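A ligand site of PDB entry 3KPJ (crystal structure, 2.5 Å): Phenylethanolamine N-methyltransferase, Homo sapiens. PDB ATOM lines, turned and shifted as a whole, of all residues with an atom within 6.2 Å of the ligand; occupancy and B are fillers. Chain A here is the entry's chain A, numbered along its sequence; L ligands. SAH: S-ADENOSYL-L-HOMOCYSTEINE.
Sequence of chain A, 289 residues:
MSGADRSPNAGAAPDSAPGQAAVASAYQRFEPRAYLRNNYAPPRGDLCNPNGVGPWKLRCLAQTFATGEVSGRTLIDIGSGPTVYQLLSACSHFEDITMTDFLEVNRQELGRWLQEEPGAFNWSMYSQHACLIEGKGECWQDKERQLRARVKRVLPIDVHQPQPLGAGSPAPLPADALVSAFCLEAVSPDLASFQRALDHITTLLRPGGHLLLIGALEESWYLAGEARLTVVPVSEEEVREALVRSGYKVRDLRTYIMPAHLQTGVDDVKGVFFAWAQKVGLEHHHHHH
O3' of the ligand lies within hydrogen-bond range of OD1 of Asn 106, 3.3 Å away.
The backbone NH (N) of Val 159 lies within hydrogen-bond range of a nitrogen (N1) of the ligand (3.0 Å).
An oxygen (OXT) of the ligand sits at hydrogen-bond distance from the side-chain hydroxyl (OH) of Tyr 85.
A nitrogen (N6) of the ligand sits at hydrogen-bond distance from the side-chain carboxylate of Asp 158, at 3.2 Å.
O of the ligand is in hydrogen-bond range of OH of Tyr 40 (2.5 Å).
SG of Cys 183 is in hydrogen-bond range of N3 of the ligand, 3.6 Å away.
An oxygen (O2') of the ligand is in hydrogen-bond range of the side-chain carboxylate (OD2) of Asp 101 (2.8 Å).
The side-chain hydroxyl of Thr 83 lies close to an oxygen (O) of the ligand, at 3.5 Å.
The backbone carbonyl oxygen (O) of Ser 80 lies close to a nitrogen (N) of the ligand (3.2 Å).
A nitrogen (N) of the ligand is in hydrogen-bond range of the backbone carbonyl oxygen (O) of Gly 79, 2.7 Å away.
The side-chain hydroxyl of Tyr 35 lies within hydrogen-bond range of an oxygen (O) of the ligand (2.8 Å).
The backbone carbonyl oxygen (O) of Ala 181 sits at hydrogen-bond distance from a nitrogen (N) of the ligand.
The backbone carbonyl oxygen (O) of Phe 182 sits close to a sulfur (SD) of the ligand (3.6 Å).
Residues that only touch the ligand: Tyr 27 (3.6 Å), Phe 30 (3.9 Å), Gly 81 (3.3 Å), Gln 86 (3.95 Å), Phe 102 (3.3 Å), Leu 103 (3.7 Å), Ile 157 (3.6 Å), His 160 (3.5 Å), Val 187 (3.1 Å) and Tyr 222 (3.997 Å).
O of Ala 186 lies within hydrogen-bond range of OH of Tyr 27, at 2.7 Å.
The side-chain amide oxygen (OD1) of Asn 106 lies close to the side-chain carboxylate (OD2) of Asp 101.
The side-chain hydroxyl of Tyr 27 is in hydrogen-bond range of the side-chain hydroxyl of Tyr 222 (3.1 Å).
The side-chain hydroxyl (OG1) of Thr 83 is in hydrogen-bond range of the backbone carbonyl oxygen (O) of Ser 80 (3.0 Å).
NE2 of His 160 sits close to O of Val 187, at 3.2 Å.
NZ of Lys 57 sits at hydrogen-bond distance from OH of Tyr 40.
The side-chain carboxylate (OD1) of Asp 158 sits at hydrogen-bond distance from the backbone NH (N) of His 160, at 2.7 Å.
The side-chain amide nitrogen of Gln 86 sits at hydrogen-bond distance from the backbone carbonyl oxygen of Thr 83 (2.8 Å).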
ATOM      1  N   ALA A  24     -34.454  39.825   2.651  1.00  0.00           N
ATOM      2  CA  ALA A  24     -33.124  39.253   2.813  1.00  0.00           C
ATOM      3  C   ALA A  24     -32.419  39.738   4.083  1.00  0.00           C
ATOM      4  O   ALA A  24     -31.292  39.329   4.378  1.00  0.00           O
ATOM      5  CB  ALA A  24     -32.254  39.527   1.578  1.00  0.00           C
ATOM      6  N   TYR A  27     -31.620  37.041   6.814  1.00  0.00           N
ATOM      7  CA  TYR A  27     -30.369  36.286   6.754  1.00  0.00           C
ATOM      8  C   TYR A  27     -29.313  36.859   7.688  1.00  0.00           C
ATOM      9  O   TYR A  27     -28.253  36.267   7.891  1.00  0.00           O
ATOM     10  CB  TYR A  27     -29.853  36.157   5.315  1.00  0.00           C
ATOM     11  CG  TYR A  27     -30.439  34.964   4.584  1.00  0.00           C
ATOM     12  CD1 TYR A  27     -31.402  35.121   3.586  1.00  0.00           C
ATOM     13  CD2 TYR A  27     -30.046  33.671   4.902  1.00  0.00           C
ATOM     14  CE1 TYR A  27     -31.941  34.027   2.929  1.00  0.00           C
ATOM     15  CE2 TYR A  27     -30.579  32.574   4.258  1.00  0.00           C
ATOM     16  CZ  TYR A  27     -31.524  32.748   3.273  1.00  0.00           C
ATOM     17  OH  TYR A  27     -32.032  31.640   2.655  1.00  0.00           O
ATOM     18  N   PHE A  30     -29.011  34.791  10.727  1.00  0.00           N
ATOM     19  CA  PHE A  30     -28.607  33.430  10.352  1.00  0.00           C
ATOM     20  C   PHE A  30     -27.366  32.931  11.098  1.00  0.00           C
ATOM     21  O   PHE A  30     -26.291  33.504  10.949  1.00  0.00           O
ATOM     22  CB  PHE A  30     -28.341  33.386   8.842  1.00  0.00           C
ATOM     23  CG  PHE A  30     -28.000  32.022   8.317  1.00  0.00           C
ATOM     24  CD1 PHE A  30     -28.997  31.192   7.823  1.00  0.00           C
ATOM     25  CD2 PHE A  30     -26.689  31.581   8.280  1.00  0.00           C
ATOM     26  CE1 PHE A  30     -28.692  29.953   7.321  1.00  0.00           C
ATOM     27  CE2 PHE A  30     -26.379  30.334   7.781  1.00  0.00           C
ATOM     28  CZ  PHE A  30     -27.381  29.516   7.293  1.00  0.00           C
ATOM     29  N   TYR A  35     -27.658  26.044  11.828  1.00  0.00           N
ATOM     30  CA  TYR A  35     -28.030  25.455  10.548  1.00  0.00           C
ATOM     31  C   TYR A  35     -27.366  24.079  10.368  1.00  0.00           C
ATOM     32  O   TYR A  35     -28.031  23.057  10.198  1.00  0.00           O
ATOM     33  CB  TYR A  35     -27.654  26.396   9.407  1.00  0.00           C
ATOM     34  CG  TYR A  35     -27.912  25.826   8.027  1.00  0.00           C
ATOM     35  CD1 TYR A  35     -29.187  25.876   7.470  1.00  0.00           C
ATOM     36  CD2 TYR A  35     -26.890  25.222   7.295  1.00  0.00           C
ATOM     37  CE1 TYR A  35     -29.432  25.364   6.206  1.00  0.00           C
ATOM     38  CE2 TYR A  35     -27.127  24.710   6.020  1.00  0.00           C
ATOM     39  CZ  TYR A  35     -28.406  24.780   5.487  1.00  0.00           C
ATOM     40  OH  TYR A  35     -28.664  24.279   4.241  1.00  0.00           O
ATOM     41  N   ASN A  39     -29.322  20.335  10.048  1.00  0.00           N
ATOM     42  CA  ASN A  39     -29.369  19.638   8.761  1.00  0.00           C
ATOM     43  C   ASN A  39     -28.303  18.604   8.503  1.00  0.00           C
ATOM     44  O   ASN A  39     -28.437  17.781   7.592  1.00  0.00           O
ATOM     45  CB  ASN A  39     -29.320  20.650   7.633  1.00  0.00           C
ATOM     46  CG  ASN A  39     -30.498  21.536   7.622  1.00  0.00           C
ATOM     47  OD1 ASN A  39     -31.636  21.076   7.592  1.00  0.00           O
ATOM     48  ND2 ASN A  39     -30.251  22.838   7.660  1.00  0.00           N
ATOM     49  N   TYR A  40     -27.220  18.664   9.259  1.00  0.00           N
ATOM     50  CA  TYR A  40     -26.035  17.866   8.957  1.00  0.00           C
ATOM     51  C   TYR A  40     -25.514  17.131  10.194  1.00  0.00           C
ATOM     52  O   TYR A  40     -24.489  16.469  10.134  1.00  0.00           O
ATOM     53  CB  TYR A  40     -24.973  18.736   8.272  1.00  0.00           C
ATOM     54  CG  TYR A  40     -25.501  19.304   6.978  1.00  0.00           C
ATOM     55  CD1 TYR A  40     -26.096  20.563   6.923  1.00  0.00           C
ATOM     56  CD2 TYR A  40     -25.478  18.540   5.816  1.00  0.00           C
ATOM     57  CE1 TYR A  40     -26.613  21.057   5.738  1.00  0.00           C
ATOM     58  CE2 TYR A  40     -25.973  19.035   4.629  1.00  0.00           C
ATOM     59  CZ  TYR A  40     -26.553  20.274   4.594  1.00  0.00           C
ATOM     60  OH  TYR A  40     -27.066  20.752   3.394  1.00  0.00           O
ATOM     61  N   LYS A  57     -28.424  12.624  -1.461  1.00  0.00           N
ATOM     62  CA  LYS A  57     -27.768  13.761  -2.086  1.00  0.00           C
ATOM     63  C   LYS A  57     -26.406  13.346  -2.651  1.00  0.00           C
ATOM     64  O   LYS A  57     -26.141  13.578  -3.836  1.00  0.00           O
ATOM     65  CB  LYS A  57     -27.682  14.945  -1.115  1.00  0.00           C
ATOM     66  CG  LYS A  57     -29.068  15.593  -0.860  1.00  0.00           C
ATOM     67  CD  LYS A  57     -28.980  16.893  -0.038  1.00  0.00           C
ATOM     68  CE  LYS A  57     -28.378  16.627   1.349  1.00  0.00           C
ATOM     69  NZ  LYS A  57     -28.272  17.854   2.181  1.00  0.00           N
ATOM     70  N   ASP A  77     -19.253  27.063  -6.824  1.00  0.00           N
ATOM     71  CA  ASP A  77     -20.333  26.661  -5.929  1.00  0.00           C
ATOM     72  C   ASP A  77     -21.106  27.890  -5.450  1.00  0.00           C
ATOM     73  O   ASP A  77     -20.605  28.686  -4.660  1.00  0.00           O
ATOM     74  CB  ASP A  77     -19.807  25.877  -4.725  1.00  0.00           C
ATOM     75  CG  ASP A  77     -20.926  25.350  -3.828  1.00  0.00           C
ATOM     76  OD1 ASP A  77     -22.067  25.248  -4.322  1.00  0.00           O
ATOM     77  OD2 ASP A  77     -20.662  25.046  -2.642  1.00  0.00           O
ATOM     78  N   ILE A  78     -22.333  28.032  -5.951  1.00  0.00           N
ATOM     79  CA  ILE A  78     -23.208  29.154  -5.629  1.00  0.00           C
ATOM     80  C   ILE A  78     -23.955  28.924  -4.329  1.00  0.00           C
ATOM     81  O   ILE A  78     -24.754  27.999  -4.242  1.00  0.00           O
ATOM     82  CB  ILE A  78     -24.261  29.352  -6.751  1.00  0.00           C
ATOM     83  CG1 ILE A  78     -23.600  29.353  -8.132  1.00  0.00           C
ATOM     84  CG2 ILE A  78     -25.123  30.594  -6.494  1.00  0.00           C
ATOM     85  CD1 ILE A  78     -22.553  30.432  -8.297  1.00  0.00           C
ATOM     86  N   GLY A  79     -23.714  29.761  -3.341  1.00  0.00           N
ATOM     87  CA  GLY A  79     -24.508  29.733  -2.118  1.00  0.00           C
ATOM     88  C   GLY A  79     -24.098  28.584  -1.241  1.00  0.00           C
ATOM     89  O   GLY A  79     -24.923  27.783  -0.791  1.00  0.00           O
ATOM     90  N   SER A  80     -22.792  28.509  -1.003  1.00  0.00           N
ATOM     91  CA  SER A  80     -22.184  27.398  -0.314  1.00  0.00           C
ATOM     92  C   SER A  80     -22.674  27.271   1.106  1.00  0.00           C
ATOM     93  O   SER A  80     -22.776  26.174   1.661  1.00  0.00           O
ATOM     94  CB  SER A  80     -20.668  27.582  -0.296  1.00  0.00           C
ATOM     95  OG  SER A  80     -20.134  27.531  -1.605  1.00  0.00           O
ATOM     96  N   GLY A  81     -22.981  28.415   1.715  1.00  0.00           N
ATOM     97  CA  GLY A  81     -23.216  28.466   3.135  1.00  0.00           C
ATOM     98  C   GLY A  81     -22.025  27.923   3.913  1.00  0.00           C
ATOM     99  O   GLY A  81     -20.866  28.146   3.554  1.00  0.00           O
ATOM    100  N   PRO A  82     -22.308  27.197   5.000  1.00  0.00           N
ATOM    101  CA  PRO A  82     -21.174  26.691   5.774  1.00  0.00           C
ATOM    102  C   PRO A  82     -20.837  25.253   5.381  1.00  0.00           C
ATOM    103  O   PRO A  82     -20.255  24.561   6.203  1.00  0.00           O
ATOM    104  CB  PRO A  82     -21.716  26.716   7.216  1.00  0.00           C
ATOM    105  CG  PRO A  82     -23.210  27.079   7.108  1.00  0.00           C
ATOM    106  CD  PRO A  82     -23.591  26.948   5.669  1.00  0.00           C
ATOM    107  N   THR A  83     -21.194  24.811   4.189  1.00  0.00           N
ATOM    108  CA  THR A  83     -21.078  23.393   3.883  1.00  0.00           C
ATOM    109  C   THR A  83     -20.196  23.095   2.681  1.00  0.00           C
ATOM    110  O   THR A  83     -20.093  23.908   1.748  1.00  0.00           O
ATOM    111  CB  THR A  83     -22.450  22.724   3.659  1.00  0.00           C
ATOM    112  OG1 THR A  83     -23.068  23.286   2.491  1.00  0.00           O
ATOM    113  CG2 THR A  83     -23.340  22.932   4.868  1.00  0.00           C
ATOM    114  N   TYR A  85     -19.969  19.488   1.568  1.00  0.00           N
ATOM    115  CA  TYR A  85     -20.426  18.202   1.048  1.00  0.00           C
ATOM    116  C   TYR A  85     -20.797  18.252  -0.427  1.00  0.00           C
ATOM    117  O   TYR A  85     -20.632  17.269  -1.157  1.00  0.00           O
ATOM    118  CB  TYR A  85     -21.619  17.704   1.858  1.00  0.00           C
ATOM    119  CG  TYR A  85     -22.927  18.361   1.471  1.00  0.00           C
ATOM    120  CD1 TYR A  85     -23.724  17.815   0.472  1.00  0.00           C
ATOM    121  CD2 TYR A  85     -23.368  19.530   2.107  1.00  0.00           C
ATOM    122  CE1 TYR A  85     -24.927  18.404   0.123  1.00  0.00           C
ATOM    123  CE2 TYR A  85     -24.571  20.119   1.758  1.00  0.00           C
ATOM    124  CZ  TYR A  85     -25.344  19.550   0.757  1.00  0.00           C
ATOM    125  OH  TYR A  85     -26.538  20.111   0.387  1.00  0.00           O
ATOM    126  N   GLN A  86     -21.323  19.379  -0.874  1.00  0.00           N
ATOM    127  CA  GLN A  86     -21.783  19.452  -2.247  1.00  0.00           C
ATOM    128  C   GLN A  86     -20.624  19.336  -3.233  1.00  0.00           C
ATOM    129  O   GLN A  86     -20.847  19.151  -4.412  1.00  0.00           O
ATOM    130  CB  GLN A  86     -22.633  20.718  -2.493  1.00  0.00           C
ATOM    131  CG  GLN A  86     -21.945  22.047  -2.198  1.00  0.00           C
ATOM    132  CD  GLN A  86     -22.037  22.462  -0.737  1.00  0.00           C
ATOM    133  OE1 GLN A  86     -22.297  21.648   0.136  1.00  0.00           O
ATOM    134  NE2 GLN A  86     -21.803  23.745  -0.482  1.00  0.00           N
ATOM    135  N   THR A 100     -18.766  30.265  -2.689  1.00  0.00           N
ATOM    136  CA  THR A 100     -19.351  31.580  -2.507  1.00  0.00           C
ATOM    137  C   THR A 100     -20.441  31.515  -1.455  1.00  0.00           C
ATOM    138  O   THR A 100     -20.983  30.444  -1.180  1.00  0.00           O
ATOM    139  CB  THR A 100     -19.952  32.139  -3.827  1.00  0.00           C
ATOM    140  OG1 THR A 100     -21.202  31.498  -4.112  1.00  0.00           O
ATOM    141  CG2 THR A 100     -19.004  31.910  -4.996  1.00  0.00           C
ATOM    142  N   ASP A 101     -20.730  32.665  -0.859  1.00  0.00           N
ATOM    143  CA  ASP A 101     -21.940  32.841  -0.073  1.00  0.00           C
ATOM    144  C   ASP A 101     -22.215  34.304   0.164  1.00  0.00           C
ATOM    145  O   ASP A 101     -21.364  35.155  -0.090  1.00  0.00           O
ATOM    146  CB  ASP A 101     -21.853  32.125   1.280  1.00  0.00           C
ATOM    147  CG  ASP A 101     -23.216  31.856   1.874  1.00  0.00           C
ATOM    148  OD1 ASP A 101     -24.051  31.217   1.191  1.00  0.00           O
ATOM    149  OD2 ASP A 101     -23.462  32.293   3.025  1.00  0.00           O
ATOM    150  N   PHE A 102     -23.419  34.597   0.646  1.00  0.00           N
ATOM    151  CA  PHE A 102     -23.842  35.945   0.928  1.00  0.00           C
ATOM    152  C   PHE A 102     -23.235  36.457   2.234  1.00  0.00           C
ATOM    153  O   PHE A 102     -22.737  37.572   2.313  1.00  0.00           O
ATOM    154  CB  PHE A 102     -25.364  35.981   1.021  1.00  0.00           C
ATOM    155  CG  PHE A 102     -25.961  37.362   0.989  1.00  0.00           C
ATOM    156  CD1 PHE A 102     -25.809  38.172  -0.119  1.00  0.00           C
ATOM    157  CD2 PHE A 102     -26.707  37.820   2.060  1.00  0.00           C
ATOM    158  CE1 PHE A 102     -26.381  39.444  -0.148  1.00  0.00           C
ATOM    159  CE2 PHE A 102     -27.283  39.080   2.037  1.00  0.00           C
ATOM    160  CZ  PHE A 102     -27.122  39.898   0.936  1.00  0.00           C
ATOM    161  N   LEU A 103     -23.273  35.614   3.265  1.00  0.00           N
ATOM    162  CA  LEU A 103     -22.879  36.040   4.605  1.00  0.00           C
ATOM    163  C   LEU A 103     -21.410  35.843   4.903  1.00  0.00           C
ATOM    164  O   LEU A 103     -20.821  34.824   4.546  1.00  0.00           O
ATOM    165  CB  LEU A 103     -23.712  35.324   5.663  1.00  0.00           C
ATOM    166  CG  LEU A 103     -25.228  35.484   5.679  1.00  0.00           C
ATOM    167  CD1 LEU A 103     -25.794  34.704   6.865  1.00  0.00           C
ATOM    168  CD2 LEU A 103     -25.672  36.951   5.735  1.00  0.00           C
ATOM    169  N   ASN A 106     -20.558  32.695   7.197  1.00  0.00           N
ATOM    170  CA  ASN A 106     -20.438  31.418   6.500  1.00  0.00           C
ATOM    171  C   ASN A 106     -19.050  31.218   5.893  1.00  0.00           C
ATOM    172  O   ASN A 106     -18.457  30.143   5.998  1.00  0.00           O
ATOM    173  CB  ASN A 106     -21.499  31.320   5.410  1.00  0.00           C
ATOM    174  CG  ASN A 106     -22.866  31.019   5.964  1.00  0.00           C
ATOM    175  OD1 ASN A 106     -23.885  31.476   5.437  1.00  0.00           O
ATOM    176  ND2 ASN A 106     -22.905  30.245   7.041  1.00  0.00           N
ATOM    177  N   ILE A 157     -21.219  36.839  -2.416  1.00  0.00           N
ATOM    178  CA  ILE A 157     -22.066  36.672  -3.582  1.00  0.00           C
ATOM    179  C   ILE A 157     -23.514  37.042  -3.290  1.00  0.00           C
ATOM    180  O   ILE A 157     -24.009  36.835  -2.174  1.00  0.00           O
ATOM    181  CB  ILE A 157     -22.001  35.215  -4.110  1.00  0.00           C
ATOM    182  CG1 ILE A 157     -22.651  35.135  -5.496  1.00  0.00           C
ATOM    183  CG2 ILE A 157     -22.653  34.231  -3.126  1.00  0.00           C
ATOM    184  CD1 ILE A 157     -22.830  33.750  -6.047  1.00  0.00           C
ATOM    185  N   ASP A 158     -24.181  37.604  -4.292  1.00  0.00           N
ATOM    186  CA  ASP A 158     -25.597  37.896  -4.206  1.00  0.00           C
ATOM    187  C   ASP A 158     -26.234  37.525  -5.519  1.00  0.00           C
ATOM    188  O   ASP A 158     -25.955  38.132  -6.553  1.00  0.00           O
ATOM    189  CB  ASP A 158     -25.832  39.369  -3.887  1.00  0.00           C
ATOM    190  CG  ASP A 158     -27.313  39.726  -3.785  1.00  0.00           C
ATOM    191  OD1 ASP A 158     -28.167  38.925  -4.253  1.00  0.00           O
ATOM    192  OD2 ASP A 158     -27.638  40.804  -3.244  1.00  0.00           O
ATOM    193  N   VAL A 159     -27.095  36.511  -5.488  1.00  0.00           N
ATOM    194  CA  VAL A 159     -27.706  36.007  -6.709  1.00  0.00           C
ATOM    195  C   VAL A 159     -28.731  36.947  -7.340  1.00  0.00           C
ATOM    196  O   VAL A 159     -29.042  36.814  -8.529  1.00  0.00           O
ATOM    197  CB  VAL A 159     -28.373  34.647  -6.477  1.00  0.00           C
ATOM    198  CG1 VAL A 159     -27.310  33.605  -6.207  1.00  0.00           C
ATOM    199  CG2 VAL A 159     -29.381  34.742  -5.323  1.00  0.00           C
ATOM    200  N   HIS A 160     -29.247  37.877  -6.552  1.00  0.00           N
ATOM    201  CA  HIS A 160     -30.187  38.878  -7.050  1.00  0.00           C
ATOM    202  C   HIS A 160     -29.544  39.849  -8.050  1.00  0.00           C
ATOM    203  O   HIS A 160     -30.174  40.246  -9.024  1.00  0.00           O
ATOM    204  CB  HIS A 160     -30.795  39.662  -5.898  1.00  0.00           C
ATOM    205  CG  HIS A 160     -31.451  38.793  -4.877  1.00  0.00           C
ATOM    206  ND1 HIS A 160     -32.418  37.865  -5.198  1.00  0.00           N
ATOM    207  CD2 HIS A 160     -31.278  38.699  -3.529  1.00  0.00           C
ATOM    208  CE1 HIS A 160     -32.814  37.247  -4.100  1.00  0.00           C
ATOM    209  NE2 HIS A 160     -32.134  37.740  -3.074  1.00  0.00           N
ATOM    210  N   SER A 180     -25.070  24.278  -7.015  1.00  0.00           N
ATOM    211  CA  SER A 180     -25.802  25.044  -6.015  1.00  0.00           C
ATOM    212  C   SER A 180     -26.817  24.169  -5.295  1.00  0.00           C
ATOM    213  O   SER A 180     -27.616  23.486  -5.928  1.00  0.00           O
ATOM    214  CB  SER A 180     -26.510  26.235  -6.659  1.00  0.00           C
ATOM    215  OG  SER A 180     -27.250  26.964  -5.675  1.00  0.00           O
ATOM    216  N   ALA A 181     -26.781  24.231  -3.968  1.00  0.00           N
ATOM    217  CA  ALA A 181     -27.668  23.436  -3.135  1.00  0.00           C
ATOM    218  C   ALA A 181     -28.450  24.297  -2.132  1.00  0.00           C
ATOM    219  O   ALA A 181     -27.852  24.992  -1.312  1.00  0.00           O
ATOM    220  CB  ALA A 181     -26.875  22.347  -2.408  1.00  0.00           C
ATOM    221  N   PHE A 182     -29.779  24.243  -2.192  1.00  0.00           N
ATOM    222  CA  PHE A 182     -30.605  24.921  -1.194  1.00  0.00           C
ATOM    223  C   PHE A 182     -30.404  26.433  -1.126  1.00  0.00           C
ATOM    224  O   PHE A 182     -30.531  27.040  -0.056  1.00  0.00           O
ATOM    225  CB  PHE A 182     -30.396  24.262   0.163  1.00  0.00           C
ATOM    226  CG  PHE A 182     -30.633  22.793   0.133  1.00  0.00           C
ATOM    227  CD1 PHE A 182     -29.573  21.909   0.060  1.00  0.00           C
ATOM    228  CD2 PHE A 182     -31.928  22.307   0.076  1.00  0.00           C
ATOM    229  CE1 PHE A 182     -29.801  20.551  -0.020  1.00  0.00           C
ATOM    230  CE2 PHE A 182     -32.170  20.957   0.004  1.00  0.00           C
ATOM    231  CZ  PHE A 182     -31.104  20.073  -0.047  1.00  0.00           C
ATOM    232  N   CYS A 183     -30.127  27.057  -2.266  1.00  0.00           N
ATOM    233  CA  CYS A 183     -29.893  28.494  -2.309  1.00  0.00           C
ATOM    234  C   CYS A 183     -31.056  29.299  -2.898  1.00  0.00           C
ATOM    235  O   CYS A 183     -31.749  30.024  -2.176  1.00  0.00           O
ATOM    236  CB  CYS A 183     -28.605  28.808  -3.041  1.00  0.00           C
ATOM    237  SG  CYS A 183     -28.194  30.549  -2.995  1.00  0.00           S
ATOM    238  N   ALA A 186     -34.353  29.484  -1.451  1.00  0.00           N
ATOM    239  CA  ALA A 186     -34.257  29.958  -0.078  1.00  0.00           C
ATOM    240  C   ALA A 186     -34.004  31.452   0.018  1.00  0.00           C
ATOM    241  O   ALA A 186     -34.189  32.052   1.072  1.00  0.00           O
ATOM    242  CB  ALA A 186     -33.176  29.192   0.672  1.00  0.00           C
ATOM    243  N   VAL A 187     -33.589  32.051  -1.094  1.00  0.00           N
ATOM    244  CA  VAL A 187     -33.327  33.485  -1.125  1.00  0.00           C
ATOM    245  C   VAL A 187     -34.347  34.255  -1.988  1.00  0.00           C
ATOM    246  O   VAL A 187     -34.231  35.461  -2.187  1.00  0.00           O
ATOM    247  CB  VAL A 187     -31.888  33.803  -1.602  1.00  0.00           C
ATOM    248  CG1 VAL A 187     -30.885  33.199  -0.647  1.00  0.00           C
ATOM    249  CG2 VAL A 187     -31.661  33.273  -3.005  1.00  0.00           C
ATOM    250  N   TYR A 222     -37.579  27.684   7.022  1.00  0.00           N
ATOM    251  CA  TYR A 222     -36.677  26.850   7.797  1.00  0.00           C
ATOM    252  C   TYR A 222     -35.910  27.738   8.755  1.00  0.00           C
ATOM    253  O   TYR A 222     -35.835  28.950   8.544  1.00  0.00           O
ATOM    254  CB  TYR A 222     -35.704  26.085   6.908  1.00  0.00           C
ATOM    255  CG  TYR A 222     -34.642  26.946   6.292  1.00  0.00           C
ATOM    256  CD1 TYR A 222     -33.360  26.974   6.814  1.00  0.00           C
ATOM    257  CD2 TYR A 222     -34.921  27.756   5.189  1.00  0.00           C
ATOM    258  CE1 TYR A 222     -32.365  27.750   6.250  1.00  0.00           C
ATOM    259  CE2 TYR A 222     -33.923  28.548   4.628  1.00  0.00           C
ATOM    260  CZ  TYR A 222     -32.651  28.538   5.167  1.00  0.00           C
ATOM    261  OH  TYR A 222     -31.640  29.302   4.639  1.00  0.00           O
HETATM  262  N   SAH L   1     -25.399  25.272   0.107  1.00  0.00           N
HETATM  263  CA  SAH L   1     -25.525  24.900   1.524  1.00  0.00           C
HETATM  264  CB  SAH L   1     -26.280  25.939   2.338  1.00  0.00           C
HETATM  265  CG  SAH L   1     -27.566  26.501   1.719  1.00  0.00           C
HETATM  266  SD  SAH L   1     -28.523  27.527   2.875  1.00  0.00           S
HETATM  267  C   SAH L   1     -26.182  23.532   1.693  1.00  0.00           C
HETATM  268  O   SAH L   1     -26.506  23.159   2.811  1.00  0.00           O
HETATM  269  OXT SAH L   1     -26.401  22.795   0.726  1.00  0.00           O
HETATM  270  C5' SAH L   1     -28.780  28.886   1.691  1.00  0.00           C
HETATM  271  C4' SAH L   1     -27.623  29.875   1.715  1.00  0.00           C
HETATM  272  O4' SAH L   1     -27.859  30.955   0.829  1.00  0.00           O
HETATM  273  C3' SAH L   1     -27.368  30.490   3.086  1.00  0.00           C
HETATM  274  O3' SAH L   1     -26.139  30.024   3.599  1.00  0.00           O
HETATM  275  C2' SAH L   1     -27.302  31.979   2.829  1.00  0.00           C
HETATM  276  O2' SAH L   1     -26.231  32.624   3.490  1.00  0.00           O
HETATM  277  C1' SAH L   1     -27.151  32.067   1.330  1.00  0.00           C
HETATM  278  N9  SAH L   1     -27.716  33.319   0.817  1.00  0.00           N
HETATM  279  C8  SAH L   1     -28.586  34.161   1.460  1.00  0.00           C
HETATM  280  N7  SAH L   1     -28.852  35.194   0.629  1.00  0.00           N
HETATM  281  C5  SAH L   1     -28.168  35.028  -0.525  1.00  0.00           C
HETATM  282  C6  SAH L   1     -28.070  35.781  -1.683  1.00  0.00           C
HETATM  283  N6  SAH L   1     -28.748  36.917  -1.812  1.00  0.00           N
HETATM  284  N1  SAH L   1     -27.273  35.334  -2.717  1.00  0.00           N
HETATM  285  C2  SAH L   1     -26.561  34.159  -2.583  1.00  0.00           C
HETATM  286  N3  SAH L   1     -26.649  33.418  -1.409  1.00  0.00           N
HETATM  287  C4  SAH L   1     -27.448  33.849  -0.412  1.00  0.00           C
